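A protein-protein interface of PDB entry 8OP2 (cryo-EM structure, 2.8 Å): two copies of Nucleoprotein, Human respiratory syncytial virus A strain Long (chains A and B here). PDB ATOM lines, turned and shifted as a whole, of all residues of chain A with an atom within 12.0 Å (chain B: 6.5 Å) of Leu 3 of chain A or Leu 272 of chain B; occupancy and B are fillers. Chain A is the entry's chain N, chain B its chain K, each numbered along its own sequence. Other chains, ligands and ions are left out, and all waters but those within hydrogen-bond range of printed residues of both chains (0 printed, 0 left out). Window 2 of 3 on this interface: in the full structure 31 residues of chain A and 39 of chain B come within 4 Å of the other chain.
The side-chain amide nitrogen of Gln 278 of chain B is in hydrogen-bond range of the backbone carbonyl oxygen of Leu 272 of chain B, at 2.4 Å.
Among the printed residues, pairs that only touch across the chains: Val 6 of chain A with Lys 265 of chain B (3.0 Å), Ala 2 of chain A with Val 285 of chain B (3.2 Å), Leu 3 of chain A with Lys 265 of chain B (3.4 Å), Val 6 of chain A with Gly 261 of chain B (3.8 Å), Leu 3 of chain A with Leu 272 of chain B (3.8 Å), Lys 5 of chain A with Val 285 of chain B (3.9 Å) and Val 6 of chain A with Met 281 of chain B (3.96 Å).
Leu 272 of chain B touches just one residue of chain A: Leu 3. No residue of chain A comes within 4 Å of Ala 264 of chain B. No residue of chain A comes within 4 Å of Lys 268 of chain B. No residue of chain A comes within 4 Å of Asn 269 of chain B. No residue of chain A comes within 4 Å of Ile 270 of chain B. No residue of chain A comes within 4 Å of Met 271 of chain B. No residue of chain A comes within 4 Å of Gly 273 of chain B. No residue of chain A comes within 4 Å of Val 277 of chain B. No residue of chain A comes within 4 Å of Gln 278 of chain B. Met 281 of chain B touches just one residue of chain A: Val 6 (3.96 Å). No residue of chain A comes within 4 Å of Val 323 of chain B. Of the printed residues of chain B, Val 6 of chain A touches Gly 261, Lys 265 and Met 281. Printed residues of chain B within 4 Å of Ala 2 of chain A: Val 285 (3.2 Å). Printed residues of chain A within 4 Å of Val 285 of chain B: Ala 2 (3.2 Å) and Lys 5 (3.9 Å). Val 324 of chain B touches none of the printed residues of chain A. The nearest residue of chain B that does not touch Leu 3 of chain A is Met 281 of chain B (4.3 Å). The nearest residue of chain A that does not touch Leu 272 of chain B is Val 6 of chain A (7.2 Å). The nearest printed residue of chain A that does not touch Val 285 of chain B is Val 6 of chain A (4.5 Å).
Of the 19 printed residues of chain B, 5 touch a printed residue of chain A. Hydrophobic or aromatic side chains of chain B that line the printed part of chain A: Leu 272, Met 281 and Val 285. Of the 9 printed residues of chain A, 4 touch a printed residue of chain B. Among the printed residues, no Asp or Glu carboxylate lies within 4 Å of a Lys or Arg side-chain nitrogen of the other chain.
No position is printed for both chains. Of the 7 pairs that touch across the chains among the printed residues, none has its exchanged pair printed and touching as well.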
ATOM      1  N   ALA A   2      -2.815 -16.303  28.311  1.00  0.00           N
ATOM      2  CA  ALA A   2      -3.725 -16.812  29.331  1.00  0.00           C
ATOM      3  C   ALA A   2      -4.469 -18.040  28.827  1.00  0.00           C
ATOM      4  O   ALA A   2      -5.003 -18.042  27.723  1.00  0.00           O
ATOM      5  CB  ALA A   2      -4.707 -15.738  29.752  1.00  0.00           C
ATOM      6  N   LEU A   3      -4.509 -19.083  29.656  1.00  0.00           N
ATOM      7  CA  LEU A   3      -5.156 -20.323  29.244  1.00  0.00           C
ATOM      8  C   LEU A   3      -6.669 -20.174  29.174  1.00  0.00           C
ATOM      9  O   LEU A   3      -7.342 -21.008  28.561  1.00  0.00           O
ATOM     10  CB  LEU A   3      -4.774 -21.448  30.203  1.00  0.00           C
ATOM     11  CG  LEU A   3      -4.858 -22.869  29.656  1.00  0.00           C
ATOM     12  CD1 LEU A   3      -3.694 -23.142  28.723  1.00  0.00           C
ATOM     13  CD2 LEU A   3      -4.872 -23.870  30.793  1.00  0.00           C
ATOM     14  N   SER A   4      -7.220 -19.128  29.787  1.00  0.00           N
ATOM     15  CA  SER A   4      -8.664 -18.936  29.793  1.00  0.00           C
ATOM     16  C   SER A   4      -9.221 -18.547  28.430  1.00  0.00           C
ATOM     17  O   SER A   4     -10.429 -18.692  28.216  1.00  0.00           O
ATOM     18  CB  SER A   4      -9.048 -17.879  30.826  1.00  0.00           C
ATOM     19  OG  SER A   4      -8.838 -16.577  30.317  1.00  0.00           O
ATOM     20  N   LYS A   5      -8.389 -18.060  27.513  1.00  0.00           N
ATOM     21  CA  LYS A   5      -8.853 -17.682  26.184  1.00  0.00           C
ATOM     22  C   LYS A   5      -8.629 -18.764  25.139  1.00  0.00           C
ATOM     23  O   LYS A   5      -8.805 -18.494  23.948  1.00  0.00           O
ATOM     24  CB  LYS A   5      -8.188 -16.383  25.728  1.00  0.00           C
ATOM     25  CG  LYS A   5      -8.591 -15.172  26.542  1.00  0.00           C
ATOM     26  CD  LYS A   5      -7.657 -14.004  26.300  1.00  0.00           C
ATOM     27  CE  LYS A   5      -7.255 -13.336  27.597  1.00  0.00           C
ATOM     28  NZ  LYS A   5      -7.169 -11.854  27.453  1.00  0.00           N
ATOM     29  N   VAL A   6      -8.258 -19.974  25.547  1.00  0.00           N
ATOM     30  CA  VAL A   6      -8.186 -21.108  24.633  1.00  0.00           C
ATOM     31  C   VAL A   6      -9.591 -21.700  24.614  1.00  0.00           C
ATOM     32  O   VAL A   6      -9.888 -22.681  25.288  1.00  0.00           O
ATOM     33  CB  VAL A   6      -7.124 -22.119  25.061  1.00  0.00           C
ATOM     34  CG1 VAL A   6      -7.162 -23.356  24.185  1.00  0.00           C
ATOM     35  CG2 VAL A   6      -5.755 -21.484  25.018  1.00  0.00           C
ATOM     36  N   LYS A   7     -10.471 -21.091  23.826  1.00  0.00           N
ATOM     37  CA  LYS A   7     -11.865 -21.499  23.797  1.00  0.00           C
ATOM     38  C   LYS A   7     -12.439 -21.252  22.413  1.00  0.00           C
ATOM     39  O   LYS A   7     -11.984 -20.370  21.681  1.00  0.00           O
ATOM     40  CB  LYS A   7     -12.684 -20.760  24.863  1.00  0.00           C
ATOM     41  CG  LYS A   7     -13.042 -19.339  24.496  1.00  0.00           C
ATOM     42  CD  LYS A   7     -14.026 -18.725  25.465  1.00  0.00           C
ATOM     43  CE  LYS A   7     -13.312 -18.121  26.656  1.00  0.00           C
ATOM     44  NZ  LYS A   7     -12.617 -16.861  26.273  1.00  0.00           N
ATOM     45  N   LEU A   8     -13.447 -22.047  22.061  1.00  0.00           N
ATOM     46  CA  LEU A   8     -14.125 -21.956  20.775  1.00  0.00           C
ATOM     47  C   LEU A   8     -15.618 -22.100  21.002  1.00  0.00           C
ATOM     48  O   LEU A   8     -16.060 -23.054  21.648  1.00  0.00           O
ATOM     49  CB  LEU A   8     -13.634 -23.032  19.805  1.00  0.00           C
ATOM     50  CG  LEU A   8     -12.538 -22.617  18.829  1.00  0.00           C
ATOM     51  CD1 LEU A   8     -11.997 -23.832  18.116  1.00  0.00           C
ATOM     52  CD2 LEU A   8     -13.076 -21.608  17.838  1.00  0.00           C
ATOM     53  N   ALA A 279     -15.999 -30.643  33.225  1.00  0.00           N
ATOM     54  CA  ALA A 279     -15.262 -30.402  31.990  1.00  0.00           C
ATOM     55  C   ALA A 279     -16.199 -29.982  30.867  1.00  0.00           C
ATOM     56  O   ALA A 279     -15.888 -29.069  30.095  1.00  0.00           O
ATOM     57  CB  ALA A 279     -14.475 -31.650  31.594  1.00  0.00           C
ATOM     58  N   GLU A 282     -18.891 -26.057  30.164  1.00  0.00           N
ATOM     59  CA  GLU A 282     -18.747 -24.864  29.331  1.00  0.00           C
ATOM     60  C   GLU A 282     -19.621 -24.960  28.085  1.00  0.00           C
ATOM     61  O   GLU A 282     -20.427 -24.066  27.797  1.00  0.00           O
ATOM     62  CB  GLU A 282     -17.284 -24.656  28.938  1.00  0.00           C
ATOM     63  CG  GLU A 282     -16.383 -24.140  30.051  1.00  0.00           C
ATOM     64  CD  GLU A 282     -16.105 -25.179  31.119  1.00  0.00           C
ATOM     65  OE1 GLU A 282     -15.698 -26.306  30.763  1.00  0.00           O
ATOM     66  OE2 GLU A 282     -16.293 -24.872  32.316  1.00  0.00           O
ATOM     67  N   GLY B 261      -7.100 -28.677  21.633  1.00  0.00           N
ATOM     68  CA  GLY B 261      -6.491 -27.743  22.564  1.00  0.00           C
ATOM     69  C   GLY B 261      -7.482 -27.214  23.579  1.00  0.00           C
ATOM     70  O   GLY B 261      -7.160 -27.081  24.764  1.00  0.00           O
ATOM     71  N   ALA B 264      -7.802 -30.007  26.009  1.00  0.00           N
ATOM     72  CA  ALA B 264      -6.674 -30.101  26.930  1.00  0.00           C
ATOM     73  C   ALA B 264      -6.728 -29.001  27.977  1.00  0.00           C
ATOM     74  O   ALA B 264      -6.275 -29.189  29.110  1.00  0.00           O
ATOM     75  CB  ALA B 264      -5.355 -30.044  26.162  1.00  0.00           C
ATOM     76  N   LYS B 265      -7.265 -27.839  27.612  1.00  0.00           N
ATOM     77  CA  LYS B 265      -7.502 -26.809  28.615  1.00  0.00           C
ATOM     78  C   LYS B 265      -8.586 -27.251  29.592  1.00  0.00           C
ATOM     79  O   LYS B 265      -8.487 -26.996  30.797  1.00  0.00           O
ATOM     80  CB  LYS B 265      -7.881 -25.492  27.939  1.00  0.00           C
ATOM     81  CG  LYS B 265      -8.101 -24.331  28.892  1.00  0.00           C
ATOM     82  CD  LYS B 265      -9.550 -24.141  29.278  1.00  0.00           C
ATOM     83  CE  LYS B 265     -10.360 -23.619  28.122  1.00  0.00           C
ATOM     84  NZ  LYS B 265     -11.786 -23.407  28.477  1.00  0.00           N
ATOM     85  N   SER B 266      -9.630 -27.914  29.089  1.00  0.00           N
ATOM     86  CA  SER B 266     -10.750 -28.294  29.945  1.00  0.00           C
ATOM     87  C   SER B 266     -10.353 -29.355  30.963  1.00  0.00           C
ATOM     88  O   SER B 266     -10.721 -29.261  32.138  1.00  0.00           O
ATOM     89  CB  SER B 266     -11.918 -28.782  29.093  1.00  0.00           C
ATOM     90  OG  SER B 266     -12.461 -27.720  28.333  1.00  0.00           O
ATOM     91  N   LYS B 268      -7.452 -29.746  32.039  1.00  0.00           N
ATOM     92  CA  LYS B 268      -6.474 -29.088  32.904  1.00  0.00           C
ATOM     93  C   LYS B 268      -5.171 -29.880  32.974  1.00  0.00           C
ATOM     94  O   LYS B 268      -4.629 -30.134  34.050  1.00  0.00           O
ATOM     95  CB  LYS B 268      -7.062 -28.867  34.297  1.00  0.00           C
ATOM     96  CG  LYS B 268      -8.167 -27.836  34.297  1.00  0.00           C
ATOM     97  CD  LYS B 268      -8.493 -27.309  35.670  1.00  0.00           C
ATOM     98  CE  LYS B 268      -9.483 -26.165  35.555  1.00  0.00           C
ATOM     99  NZ  LYS B 268      -8.978 -25.107  34.638  1.00  0.00           N
ATOM    100  N   ASN B 269      -4.674 -30.275  31.807  1.00  0.00           N
ATOM    101  CA  ASN B 269      -3.422 -31.013  31.733  1.00  0.00           C
ATOM    102  C   ASN B 269      -2.286 -30.171  32.299  1.00  0.00           C
ATOM    103  O   ASN B 269      -2.198 -28.968  32.035  1.00  0.00           O
ATOM    104  CB  ASN B 269      -3.134 -31.417  30.290  1.00  0.00           C
ATOM    105  CG  ASN B 269      -2.076 -32.486  30.186  1.00  0.00           C
ATOM    106  OD1 ASN B 269      -0.975 -32.332  30.702  1.00  0.00           O
ATOM    107  ND2 ASN B 269      -2.402 -33.581  29.515  1.00  0.00           N
ATOM    108  N   ILE B 270      -1.424 -30.801  33.098  1.00  0.00           N
ATOM    109  CA  ILE B 270      -0.375 -30.057  33.785  1.00  0.00           C
ATOM    110  C   ILE B 270       0.708 -29.595  32.823  1.00  0.00           C
ATOM    111  O   ILE B 270       1.287 -28.517  33.010  1.00  0.00           O
ATOM    112  CB  ILE B 270       0.210 -30.896  34.935  1.00  0.00           C
ATOM    113  CG1 ILE B 270       0.824 -32.192  34.405  1.00  0.00           C
ATOM    114  CG2 ILE B 270      -0.849 -31.168  35.985  1.00  0.00           C
ATOM    115  CD1 ILE B 270       1.764 -32.836  35.369  1.00  0.00           C
ATOM    116  N   MET B 271       1.005 -30.380  31.784  1.00  0.00           N
ATOM    117  CA  MET B 271       2.075 -29.999  30.871  1.00  0.00           C
ATOM    118  C   MET B 271       1.762 -28.744  30.069  1.00  0.00           C
ATOM    119  O   MET B 271       2.580 -28.348  29.233  1.00  0.00           O
ATOM    120  CB  MET B 271       2.406 -31.156  29.934  1.00  0.00           C
ATOM    121  CG  MET B 271       2.753 -32.434  30.674  1.00  0.00           C
ATOM    122  SD  MET B 271       4.266 -32.243  31.633  1.00  0.00           S
ATOM    123  CE  MET B 271       4.128 -33.593  32.803  1.00  0.00           C
ATOM    124  N   LEU B 272       0.606 -28.124  30.288  1.00  0.00           N
ATOM    125  CA  LEU B 272       0.382 -26.778  29.784  1.00  0.00           C
ATOM    126  C   LEU B 272       1.130 -25.740  30.606  1.00  0.00           C
ATOM    127  O   LEU B 272       1.216 -24.579  30.192  1.00  0.00           O
ATOM    128  CB  LEU B 272      -1.111 -26.458  29.773  1.00  0.00           C
ATOM    129  CG  LEU B 272      -1.996 -27.299  28.855  1.00  0.00           C
ATOM    130  CD1 LEU B 272      -3.457 -27.011  29.138  1.00  0.00           C
ATOM    131  CD2 LEU B 272      -1.662 -27.037  27.400  1.00  0.00           C
ATOM    132  N   GLY B 273       1.652 -26.126  31.766  1.00  0.00           N
ATOM    133  CA  GLY B 273       2.471 -25.290  32.613  1.00  0.00           C
ATOM    134  C   GLY B 273       3.958 -25.389  32.366  1.00  0.00           C
ATOM    135  O   GLY B 273       4.735 -24.755  33.086  1.00  0.00           O
ATOM    136  N   HIS B 274       4.381 -26.171  31.379  1.00  0.00           N
ATOM    137  CA  HIS B 274       5.790 -26.266  31.041  1.00  0.00           C
ATOM    138  C   HIS B 274       6.297 -24.919  30.531  1.00  0.00           C
ATOM    139  O   HIS B 274       5.524 -24.017  30.201  1.00  0.00           O
ATOM    140  CB  HIS B 274       6.005 -27.362  29.997  1.00  0.00           C
ATOM    141  CG  HIS B 274       7.436 -27.749  29.800  1.00  0.00           C
ATOM    142  ND1 HIS B 274       7.956 -28.069  28.563  1.00  0.00           N
ATOM    143  CD2 HIS B 274       8.456 -27.884  30.680  1.00  0.00           C
ATOM    144  CE1 HIS B 274       9.234 -28.377  28.689  1.00  0.00           C
ATOM    145  NE2 HIS B 274       9.561 -28.273  29.964  1.00  0.00           N
ATOM    146  N   ALA B 275       7.624 -24.783  30.485  1.00  0.00           N
ATOM    147  CA  ALA B 275       8.226 -23.495  30.149  1.00  0.00           C
ATOM    148  C   ALA B 275       7.977 -23.122  28.691  1.00  0.00           C
ATOM    149  O   ALA B 275       7.566 -21.997  28.389  1.00  0.00           O
ATOM    150  CB  ALA B 275       9.723 -23.531  30.449  1.00  0.00           C
ATOM    151  N   VAL B 277       5.730 -24.307  26.528  1.00  0.00           N
ATOM    152  CA  VAL B 277       4.313 -24.096  26.258  1.00  0.00           C
ATOM    153  C   VAL B 277       3.904 -22.691  26.671  1.00  0.00           C
ATOM    154  O   VAL B 277       3.201 -21.986  25.933  1.00  0.00           O
ATOM    155  CB  VAL B 277       3.473 -25.167  26.973  1.00  0.00           C
ATOM    156  CG1 VAL B 277       2.013 -25.026  26.603  1.00  0.00           C
ATOM    157  CG2 VAL B 277       3.983 -26.551  26.621  1.00  0.00           C
ATOM    158  N   GLN B 278       4.348 -22.253  27.848  1.00  0.00           N
ATOM    159  CA  GLN B 278       4.023 -20.907  28.298  1.00  0.00           C
ATOM    160  C   GLN B 278       4.714 -19.854  27.448  1.00  0.00           C
ATOM    161  O   GLN B 278       4.214 -18.731  27.325  1.00  0.00           O
ATOM    162  CB  GLN B 278       4.391 -20.746  29.769  1.00  0.00           C
ATOM    163  CG  GLN B 278       3.467 -21.496  30.694  1.00  0.00           C
ATOM    164  CD  GLN B 278       2.017 -21.139  30.461  1.00  0.00           C
ATOM    165  OE1 GLN B 278       1.646 -19.969  30.472  1.00  0.00           O
ATOM    166  NE2 GLN B 278       1.189 -22.150  30.234  1.00  0.00           N
ATOM    167  N   MET B 281       2.308 -19.544  24.516  1.00  0.00           N
ATOM    168  CA  MET B 281       0.906 -19.261  24.817  1.00  0.00           C
ATOM    169  C   MET B 281       0.430 -17.932  24.240  1.00  0.00           C
ATOM    170  O   MET B 281      -0.755 -17.785  23.925  1.00  0.00           O
ATOM    171  CB  MET B 281       0.673 -19.294  26.328  1.00  0.00           C
ATOM    172  CG  MET B 281       0.575 -20.686  26.942  1.00  0.00           C
ATOM    173  SD  MET B 281      -0.491 -21.947  26.190  1.00  0.00           S
ATOM    174  CE  MET B 281      -1.858 -21.005  25.520  1.00  0.00           C
ATOM    175  N   VAL B 285      -2.931 -17.957  21.991  1.00  0.00           N
ATOM    176  CA  VAL B 285      -4.127 -17.167  22.259  1.00  0.00           C
ATOM    177  C   VAL B 285      -4.424 -16.244  21.084  1.00  0.00           C
ATOM    178  O   VAL B 285      -5.587 -15.985  20.758  1.00  0.00           O
ATOM    179  CB  VAL B 285      -3.959 -16.388  23.574  1.00  0.00           C
ATOM    180  CG1 VAL B 285      -4.997 -15.292  23.693  1.00  0.00           C
ATOM    181  CG2 VAL B 285      -4.053 -17.333  24.747  1.00  0.00           C
ATOM    182  N   PHE B 320       3.200 -26.712  22.270  1.00  0.00           N
ATOM    183  CA  PHE B 320       1.771 -26.735  22.565  1.00  0.00           C
ATOM    184  C   PHE B 320       1.066 -27.820  21.763  1.00  0.00           C
ATOM    185  O   PHE B 320       0.201 -28.528  22.288  1.00  0.00           O
ATOM    186  CB  PHE B 320       1.162 -25.364  22.280  1.00  0.00           C
ATOM    187  CG  PHE B 320      -0.302 -25.268  22.591  1.00  0.00           C
ATOM    188  CD1 PHE B 320      -0.732 -24.995  23.874  1.00  0.00           C
ATOM    189  CD2 PHE B 320      -1.248 -25.426  21.597  1.00  0.00           C
ATOM    190  CE1 PHE B 320      -2.075 -24.896  24.159  1.00  0.00           C
ATOM    191  CE2 PHE B 320      -2.590 -25.328  21.880  1.00  0.00           C
ATOM    192  CZ  PHE B 320      -3.003 -25.063  23.161  1.00  0.00           C
ATOM    193  N   VAL B 323       1.839 -31.187  23.347  1.00  0.00           N
ATOM    194  CA  VAL B 323       1.059 -31.386  24.564  1.00  0.00           C
ATOM    195  C   VAL B 323      -0.387 -31.725  24.221  1.00  0.00           C
ATOM    196  O   VAL B 323      -1.002 -32.598  24.846  1.00  0.00           O
ATOM    197  CB  VAL B 323       1.154 -30.146  25.467  1.00  0.00           C
ATOM    198  CG1 VAL B 323       0.110 -30.202  26.563  1.00  0.00           C
ATOM    199  CG2 VAL B 323       2.535 -30.050  26.067  1.00  0.00           C
ATOM    200  N   VAL B 324      -0.951 -31.043  23.223  1.00  0.00           N
ATOM    201  CA  VAL B 324      -2.341 -31.279  22.839  1.00  0.00           C
ATOM    202  C   VAL B 324      -2.518 -32.686  22.274  1.00  0.00           C
ATOM    203  O   VAL B 324      -3.476 -33.390  22.617  1.00  0.00           O
ATOM    204  CB  VAL B 324      -2.796 -30.196  21.846  1.00  0.00           C
ATOM    205  CG1 VAL B 324      -4.037 -30.630  21.118  1.00  0.00           C
ATOM    206  CG2 VAL B 324      -3.041 -28.900  22.581  1.00  0.00           C
